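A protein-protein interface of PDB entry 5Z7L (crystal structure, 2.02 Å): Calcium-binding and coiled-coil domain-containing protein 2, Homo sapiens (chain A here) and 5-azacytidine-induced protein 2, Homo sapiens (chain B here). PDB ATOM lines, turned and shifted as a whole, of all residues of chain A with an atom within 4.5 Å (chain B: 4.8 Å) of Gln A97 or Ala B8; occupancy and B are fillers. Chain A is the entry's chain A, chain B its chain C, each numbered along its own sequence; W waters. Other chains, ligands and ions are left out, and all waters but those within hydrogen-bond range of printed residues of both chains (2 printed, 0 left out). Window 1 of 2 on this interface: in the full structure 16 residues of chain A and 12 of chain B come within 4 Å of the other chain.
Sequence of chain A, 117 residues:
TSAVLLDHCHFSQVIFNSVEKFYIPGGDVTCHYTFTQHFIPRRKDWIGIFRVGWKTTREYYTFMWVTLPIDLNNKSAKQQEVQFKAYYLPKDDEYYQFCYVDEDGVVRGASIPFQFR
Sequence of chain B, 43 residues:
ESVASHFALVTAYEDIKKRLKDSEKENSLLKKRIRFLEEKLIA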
ATOM      1  N   GLY A  48      14.046  27.555 -18.314  1.00  0.00           N
ATOM      2  CA  GLY A  48      13.133  26.484 -17.982  1.00  0.00           C
ATOM      3  C   GLY A  48      12.790  25.662 -19.209  1.00  0.00           C
ATOM      4  O   GLY A  48      12.773  26.153 -20.338  1.00  0.00           O
ATOM      5  N   ILE A  49      12.527  24.395 -18.980  1.00  0.00           N
ATOM      6  CA  ILE A  49      11.815  23.591 -19.956  1.00  0.00           C
ATOM      7  C   ILE A  49      10.339  23.693 -19.595  1.00  0.00           C
ATOM      8  O   ILE A  49       9.944  23.368 -18.466  1.00  0.00           O
ATOM      9  CB  ILE A  49      12.326  22.145 -19.954  1.00  0.00           C
ATOM     10  CG1 ILE A  49      13.825  22.153 -20.301  1.00  0.00           C
ATOM     11  CG2 ILE A  49      11.537  21.279 -20.940  1.00  0.00           C
ATOM     12  CD1 ILE A  49      14.459  20.795 -20.351  1.00  0.00           C
ATOM     13  N   PHE A  50       9.544  24.221 -20.529  1.00  0.00           N
ATOM     14  CA  PHE A  50       8.117  24.453 -20.359  1.00  0.00           C
ATOM     15  C   PHE A  50       7.338  23.618 -21.361  1.00  0.00           C
ATOM     16  O   PHE A  50       7.735  23.497 -22.527  1.00  0.00           O
ATOM     17  CB  PHE A  50       7.744  25.932 -20.592  1.00  0.00           C
ATOM     18  CG  PHE A  50       8.157  26.857 -19.488  1.00  0.00           C
ATOM     19  CD1 PHE A  50       9.438  27.401 -19.462  1.00  0.00           C
ATOM     20  CD2 PHE A  50       7.260  27.211 -18.489  1.00  0.00           C
ATOM     21  CE1 PHE A  50       9.826  28.265 -18.441  1.00  0.00           C
ATOM     22  CE2 PHE A  50       7.634  28.073 -17.466  1.00  0.00           C
ATOM     23  CZ  PHE A  50       8.923  28.601 -17.440  1.00  0.00           C
ATOM     24  N   VAL A  52       4.671  23.504 -24.019  1.00  0.00           N
ATOM     25  CA  VAL A  52       4.037  24.475 -24.893  1.00  0.00           C
ATOM     26  C   VAL A  52       2.625  24.753 -24.409  1.00  0.00           C
ATOM     27  O   VAL A  52       1.889  23.839 -24.024  1.00  0.00           O
ATOM     28  CB  VAL A  52       4.034  23.957 -26.343  1.00  0.00           C
ATOM     29  CG1 VAL A  52       3.197  24.867 -27.224  1.00  0.00           C
ATOM     30  CG2 VAL A  52       5.464  23.847 -26.868  1.00  0.00           C
ATOM     31  N   TRP A  54       2.124  26.857 -21.811  1.00  0.00           N
ATOM     32  CA  TRP A  54       2.193  27.266 -20.410  1.00  0.00           C
ATOM     33  C   TRP A  54       1.615  28.666 -20.217  1.00  0.00           C
ATOM     34  O   TRP A  54       1.688  29.526 -21.103  1.00  0.00           O
ATOM     35  CB  TRP A  54       3.642  27.241 -19.919  1.00  0.00           C
ATOM     36  CG  TRP A  54       4.542  28.134 -20.734  1.00  0.00           C
ATOM     37  CD1 TRP A  54       5.234  27.797 -21.864  1.00  0.00           C
ATOM     38  CD2 TRP A  54       4.844  29.514 -20.477  1.00  0.00           C
ATOM     39  NE1 TRP A  54       5.955  28.881 -22.319  1.00  0.00           N
ATOM     40  CE2 TRP A  54       5.737  29.943 -21.481  1.00  0.00           C
ATOM     41  CE3 TRP A  54       4.457  30.422 -19.490  1.00  0.00           C
ATOM     42  CZ2 TRP A  54       6.237  31.247 -21.530  1.00  0.00           C
ATOM     43  CZ3 TRP A  54       4.950  31.721 -19.545  1.00  0.00           C
ATOM     44  CH2 TRP A  54       5.828  32.118 -20.551  1.00  0.00           C
ATOM     45  N   TYR A  96       7.639  20.582 -25.777  1.00  0.00           N
ATOM     46  CA  TYR A  96       8.266  21.475 -24.815  1.00  0.00           C
ATOM     47  C   TYR A  96       9.078  22.530 -25.555  1.00  0.00           C
ATOM     48  O   TYR A  96       9.344  22.417 -26.757  1.00  0.00           O
ATOM     49  CB  TYR A  96       9.151  20.678 -23.852  1.00  0.00           C
ATOM     50  CG  TYR A  96       8.343  19.718 -22.996  1.00  0.00           C
ATOM     51  CD1 TYR A  96       7.852  20.109 -21.741  1.00  0.00           C
ATOM     52  CD2 TYR A  96       8.053  18.433 -23.444  1.00  0.00           C
ATOM     53  CE1 TYR A  96       7.086  19.230 -20.956  1.00  0.00           C
ATOM     54  CE2 TYR A  96       7.293  17.548 -22.664  1.00  0.00           C
ATOM     55  CZ  TYR A  96       6.811  17.962 -21.431  1.00  0.00           C
ATOM     56  OH  TYR A  96       6.073  17.093 -20.667  1.00  0.00           O
ATOM     57  N   GLN A  97       9.466  23.575 -24.830  1.00  0.00           N
ATOM     58  CA  GLN A  97      10.304  24.640 -25.372  1.00  0.00           C
ATOM     59  C   GLN A  97      11.172  25.158 -24.230  1.00  0.00           C
ATOM     60  O   GLN A  97      10.874  24.925 -23.056  1.00  0.00           O
ATOM     61  CB  GLN A  97       9.444  25.775 -25.991  1.00  0.00           C
ATOM     62  CG  GLN A  97       8.624  26.526 -24.933  1.00  0.00           C
ATOM     63  CD  GLN A  97       7.587  27.523 -25.467  1.00  0.00           C
ATOM     64  OE1 GLN A  97       6.637  27.863 -24.748  1.00  0.00           O
ATOM     65  NE2 GLN A  97       7.762  28.001 -26.707  1.00  0.00           N
ATOM     66  N   PHE A  98      12.271  25.830 -24.584  1.00  0.00           N
ATOM     67  CA  PHE A  98      13.075  26.568 -23.623  1.00  0.00           C
ATOM     68  C   PHE A  98      12.519  27.980 -23.463  1.00  0.00           C
ATOM     69  O   PHE A  98      12.151  28.635 -24.444  1.00  0.00           O
ATOM     70  CB  PHE A  98      14.540  26.665 -24.067  1.00  0.00           C
ATOM     71  CG  PHE A  98      15.223  25.323 -24.292  1.00  0.00           C
ATOM     72  CD1 PHE A  98      15.506  24.476 -23.223  1.00  0.00           C
ATOM     73  CD2 PHE A  98      15.620  24.933 -25.579  1.00  0.00           C
ATOM     74  CE1 PHE A  98      16.154  23.258 -23.419  1.00  0.00           C
ATOM     75  CE2 PHE A  98      16.264  23.709 -25.794  1.00  0.00           C
ATOM     76  CZ  PHE A  98      16.527  22.866 -24.718  1.00  0.00           C
ATOM     77  N   CYS A  99      12.465  28.451 -22.221  1.00  0.00           N
ATOM     78  CA  CYS A  99      12.251  29.867 -21.940  1.00  0.00           C
ATOM     79  C   CYS A  99      13.288  30.374 -20.954  1.00  0.00           C
ATOM     80  O   CYS A  99      13.527  29.752 -19.912  1.00  0.00           O
ATOM     81  CB  CYS A  99      10.829  30.159 -21.421  1.00  0.00           C
ATOM     82  SG  CYS A  99       9.489  29.484 -22.474  1.00  0.00           S
ATOM     83  N   ALA A 110      12.132  32.579 -25.857  1.00  0.00           N
ATOM     84  CA  ALA A 110      11.323  31.366 -25.918  1.00  0.00           C
ATOM     85  C   ALA A 110      11.745  30.616 -27.171  1.00  0.00           C
ATOM     86  O   ALA A 110      11.888  31.232 -28.231  1.00  0.00           O
ATOM     87  CB  ALA A 110       9.812  31.705 -25.953  1.00  0.00           C
ATOM     88  N   SER A 111      11.966  29.315 -27.057  1.00  0.00           N
ATOM     89  CA  SER A 111      12.507  28.565 -28.180  1.00  0.00           C
ATOM     90  C   SER A 111      11.383  27.955 -29.021  1.00  0.00           C
ATOM     91  O   SER A 111      10.212  27.913 -28.619  1.00  0.00           O
ATOM     92  CB  SER A 111      13.430  27.453 -27.685  1.00  0.00           C
ATOM     93  OG  SER A 111      12.673  26.336 -27.212  1.00  0.00           O
ATOM     94  N   ILE A 112      11.755  27.471 -30.203  1.00  0.00           N
ATOM     95  CA  ILE A 112      10.879  26.603 -30.981  1.00  0.00           C
ATOM     96  C   ILE A 112      10.741  25.301 -30.197  1.00  0.00           C
ATOM     97  O   ILE A 112      11.592  24.996 -29.346  1.00  0.00           O
ATOM     98  CB  ILE A 112      11.420  26.364 -32.400  1.00  0.00           C
ATOM     99  CG1 ILE A 112      12.767  25.629 -32.358  1.00  0.00           C
ATOM    100  CG2 ILE A 112      11.532  27.683 -33.183  1.00  0.00           C
ATOM    101  CD1 ILE A 112      13.352  25.441 -33.783  1.00  0.00           C
ATOM    102  N   PRO A 113       9.688  24.520 -30.411  1.00  0.00           N
ATOM    103  CA  PRO A 113       9.417  23.398 -29.518  1.00  0.00           C
ATOM    104  C   PRO A 113      10.052  22.095 -29.985  1.00  0.00           C
ATOM    105  O   PRO A 113      10.492  21.949 -31.130  1.00  0.00           O
ATOM    106  CB  PRO A 113       7.889  23.301 -29.549  1.00  0.00           C
ATOM    107  CG  PRO A 113       7.542  23.734 -30.929  1.00  0.00           C
ATOM    108  CD  PRO A 113       8.568  24.759 -31.343  1.00  0.00           C
ATOM    109  N   PHE A 114      10.089  21.142 -29.053  1.00  0.00           N
ATOM    110  CA  PHE A 114      10.728  19.850 -29.249  1.00  0.00           C
ATOM    111  C   PHE A 114       9.989  18.815 -28.419  1.00  0.00           C
ATOM    112  O   PHE A 114       9.198  19.139 -27.528  1.00  0.00           O
ATOM    113  CB  PHE A 114      12.209  19.871 -28.847  1.00  0.00           C
ATOM    114  CG  PHE A 114      12.467  20.599 -27.560  1.00  0.00           C
ATOM    115  CD1 PHE A 114      12.303  19.963 -26.337  1.00  0.00           C
ATOM    116  CD2 PHE A 114      12.856  21.929 -27.572  1.00  0.00           C
ATOM    117  CE1 PHE A 114      12.523  20.642 -25.149  1.00  0.00           C
ATOM    118  CE2 PHE A 114      13.075  22.616 -26.390  1.00  0.00           C
ATOM    119  CZ  PHE A 114      12.916  21.965 -25.175  1.00  0.00           C
ATOM    120  N   ALA B   4       4.006  37.443 -22.472  1.00  0.00           N
ATOM    121  CA  ALA B   4       5.073  36.485 -22.739  1.00  0.00           C
ATOM    122  C   ALA B   4       4.496  35.100 -23.002  1.00  0.00           C
ATOM    123  O   ALA B   4       4.949  34.400 -23.912  1.00  0.00           O
ATOM    124  CB  ALA B   4       6.066  36.460 -21.573  1.00  0.00           C
ATOM    125  N   SER B   5       3.471  34.705 -22.238  1.00  0.00           N
ATOM    126  CA  SER B   5       2.853  33.396 -22.440  1.00  0.00           C
ATOM    127  C   SER B   5       2.335  33.247 -23.860  1.00  0.00           C
ATOM    128  O   SER B   5       2.546  32.218 -24.515  1.00  0.00           O
ATOM    129  CB  SER B   5       1.710  33.188 -21.446  1.00  0.00           C
ATOM    130  OG  SER B   5       0.956  32.039 -21.807  1.00  0.00           O
ATOM    131  N   HIS B   6       1.633  34.270 -24.348  1.00  0.00           N
ATOM    132  CA  HIS B   6       1.079  34.217 -25.690  1.00  0.00           C
ATOM    133  C   HIS B   6       2.190  34.231 -26.724  1.00  0.00           C
ATOM    134  O   HIS B   6       2.182  33.442 -27.678  1.00  0.00           O
ATOM    135  CB  HIS B   6       0.134  35.394 -25.892  1.00  0.00           C
ATOM    136  CG  HIS B   6      -0.536  35.398 -27.221  1.00  0.00           C
ATOM    137  ND1 HIS B   6       0.085  35.860 -28.361  1.00  0.00           N
ATOM    138  CD2 HIS B   6      -1.778  35.010 -27.592  1.00  0.00           C
ATOM    139  CE1 HIS B   6      -0.751  35.755 -29.381  1.00  0.00           C
ATOM    140  NE2 HIS B   6      -1.887  35.244 -28.940  1.00  0.00           N
ATOM    141  N   PHE B   7       3.162  35.129 -26.546  1.00  0.00           N
ATOM    142  CA  PHE B   7       4.311  35.169 -27.445  1.00  0.00           C
ATOM    143  C   PHE B   7       5.005  33.811 -27.536  1.00  0.00           C
ATOM    144  O   PHE B   7       5.371  33.361 -28.631  1.00  0.00           O
ATOM    145  CB  PHE B   7       5.296  36.237 -26.970  1.00  0.00           C
ATOM    146  CG  PHE B   7       6.529  36.331 -27.815  1.00  0.00           C
ATOM    147  CD1 PHE B   7       6.520  37.051 -28.999  1.00  0.00           C
ATOM    148  CD2 PHE B   7       7.697  35.692 -27.434  1.00  0.00           C
ATOM    149  CE1 PHE B   7       7.656  37.133 -29.784  1.00  0.00           C
ATOM    150  CE2 PHE B   7       8.831  35.773 -28.217  1.00  0.00           C
ATOM    151  CZ  PHE B   7       8.809  36.496 -29.390  1.00  0.00           C
ATOM    152  N   ALA B   8       5.216  33.149 -26.394  1.00  0.00           N
ATOM    153  CA  ALA B   8       5.931  31.883 -26.423  1.00  0.00           C
ATOM    154  C   ALA B   8       5.145  30.833 -27.181  1.00  0.00           C
ATOM    155  O   ALA B   8       5.738  29.983 -27.850  1.00  0.00           O
ATOM    156  CB  ALA B   8       6.222  31.394 -25.005  1.00  0.00           C
ATOM    157  N   LEU B   9       3.810  30.890 -27.095  1.00  0.00           N
ATOM    158  CA  LEU B   9       2.983  29.931 -27.810  1.00  0.00           C
ATOM    159  C   LEU B   9       2.967  30.231 -29.303  1.00  0.00           C
ATOM    160  O   LEU B   9       2.953  29.306 -30.125  1.00  0.00           O
ATOM    161  CB  LEU B   9       1.566  29.946 -27.226  1.00  0.00           C
ATOM    162  CG  LEU B   9       0.519  29.003 -27.838  1.00  0.00           C
ATOM    163  CD1 LEU B   9       0.993  27.550 -27.828  1.00  0.00           C
ATOM    164  CD2 LEU B   9      -0.816  29.143 -27.103  1.00  0.00           C
ATOM    165  N   VAL B  10       2.935  31.518 -29.670  1.00  0.00           N
ATOM    166  CA  VAL B  10       3.057  31.913 -31.073  1.00  0.00           C
ATOM    167  C   VAL B  10       4.354  31.366 -31.648  1.00  0.00           C
ATOM    168  O   VAL B  10       4.378  30.768 -32.731  1.00  0.00           O
ATOM    169  CB  VAL B  10       2.983  33.449 -31.212  1.00  0.00           C
ATOM    170  CG1 VAL B  10       3.455  33.911 -32.600  1.00  0.00           C
ATOM    171  CG2 VAL B  10       1.578  33.955 -30.940  1.00  0.00           C
ATOM    172  N   THR B  11       5.451  31.541 -30.913  1.00  0.00           N
ATOM    173  CA  THR B  11       6.726  30.962 -31.323  1.00  0.00           C
ATOM    174  C   THR B  11       6.609  29.458 -31.556  1.00  0.00           C
ATOM    175  O   THR B  11       7.079  28.938 -32.573  1.00  0.00           O
ATOM    176  CB  THR B  11       7.792  31.258 -30.265  1.00  0.00           C
ATOM    177  OG1 THR B  11       7.999  32.667 -30.190  1.00  0.00           O
ATOM    178  CG2 THR B  11       9.129  30.575 -30.624  1.00  0.00           C
ATOM    179  N   ALA B  12       6.004  28.735 -30.614  1.00  0.00           N
ATOM    180  CA  ALA B  12       5.809  27.298 -30.822  1.00  0.00           C
ATOM    181  C   ALA B  12       4.947  27.029 -32.048  1.00  0.00           C
ATOM    182  O   ALA B  12       5.317  26.240 -32.925  1.00  0.00           O
ATOM    183  CB  ALA B  12       5.180  26.655 -29.588  1.00  0.00           C
HETATM  184  O   HOH W   1       3.981  28.036 -25.187  1.00  0.00           O
HETATM  185  O   HOH W   2       2.326  29.613 -23.711  1.00  0.00           O
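The backbone carbonyl oxygen of Trp A54 lies within hydrogen-bond range of the side-chain hydroxyl of Ser B5, 2.7 Å away. NE2 of Gln A97 is in hydrogen-bond range of O of Ala B8.
Among the printed residues, pairs that only touch across the chains: Trp A54 with Ala B8 (3.5 Å), Ser A111 with Thr B11 (3.5 Å), Val A52 with Leu B9 (3.5 Å), Val A52 with Ala B12 (3.6 Å), Ala A110 with Thr B11 (3.7 Å), Ala A110 with Ala B8 (3.7 Å) and Pro A113 with Ala B12 (3.8 Å).
Water W2 lies within hydrogen-bond range of the backbone carbonyl oxygen (O) of Trp A54 (2.7 Å) and the backbone carbonyl oxygen (O) of Ser B5 (2.7 Å). Water W1 lies within hydrogen-bond range of OE1 of Gln A97 (2.7 Å) and N of Leu B9 (3.4 Å).
Printed residues of chain A within 4 Å of Ala B8: Trp A54 (3.5 Å), Gln A97 (3.1 Å) and Ala A110 (3.7 Å). Of the printed residues of chain B, Ala A110 touches Ala B8 (3.7 Å) and Thr B11 (3.7 Å). Printed residues of chain B within 4 Å of Val A52: Leu B9 and Ala B12. Of the printed residues of chain B, Trp A54 touches Ser B5 (2.7 Å) and Ala B8 (3.5 Å). Of the printed residues of chain A, Thr B11 touches Ala A110 (3.7 Å) and Ser A111 (3.5 Å). Tyr A96 touches none of the printed residues of chain B. Gly A48 touches none of the printed residues of chain B. The nearest residue of chain B that does not touch Gln A97 is Ala B12 (4.1 Å). The nearest printed residue of chain A that does not touch Ala B8 is Cys A99 (4.6 Å).
The backbone NH (N) of Gln A97 is in hydrogen-bond range of the backbone carbonyl oxygen (O) of Phe A50 (2.9 Å). The indole nitrogen of Trp A54 lies within hydrogen-bond range of the side-chain amide oxygen of Gln A97, at 2.7 Å. NE1 of Trp A54 sits at hydrogen-bond distance from SG of Cys A99, at 3.6 Å. O of Ser A111 is in hydrogen-bond range of NE2 of Gln A97, 3.1 Å away. The backbone carbonyl oxygen (O) of Phe A98 lies within hydrogen-bond range of the backbone NH (N) of Ser A111, at 2.7 Å. O of Phe B7 is in hydrogen-bond range of OG1 of Thr B11 (3.1 Å).
Of the 14 printed residues of chain A, 6 touch a printed residue of chain B.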
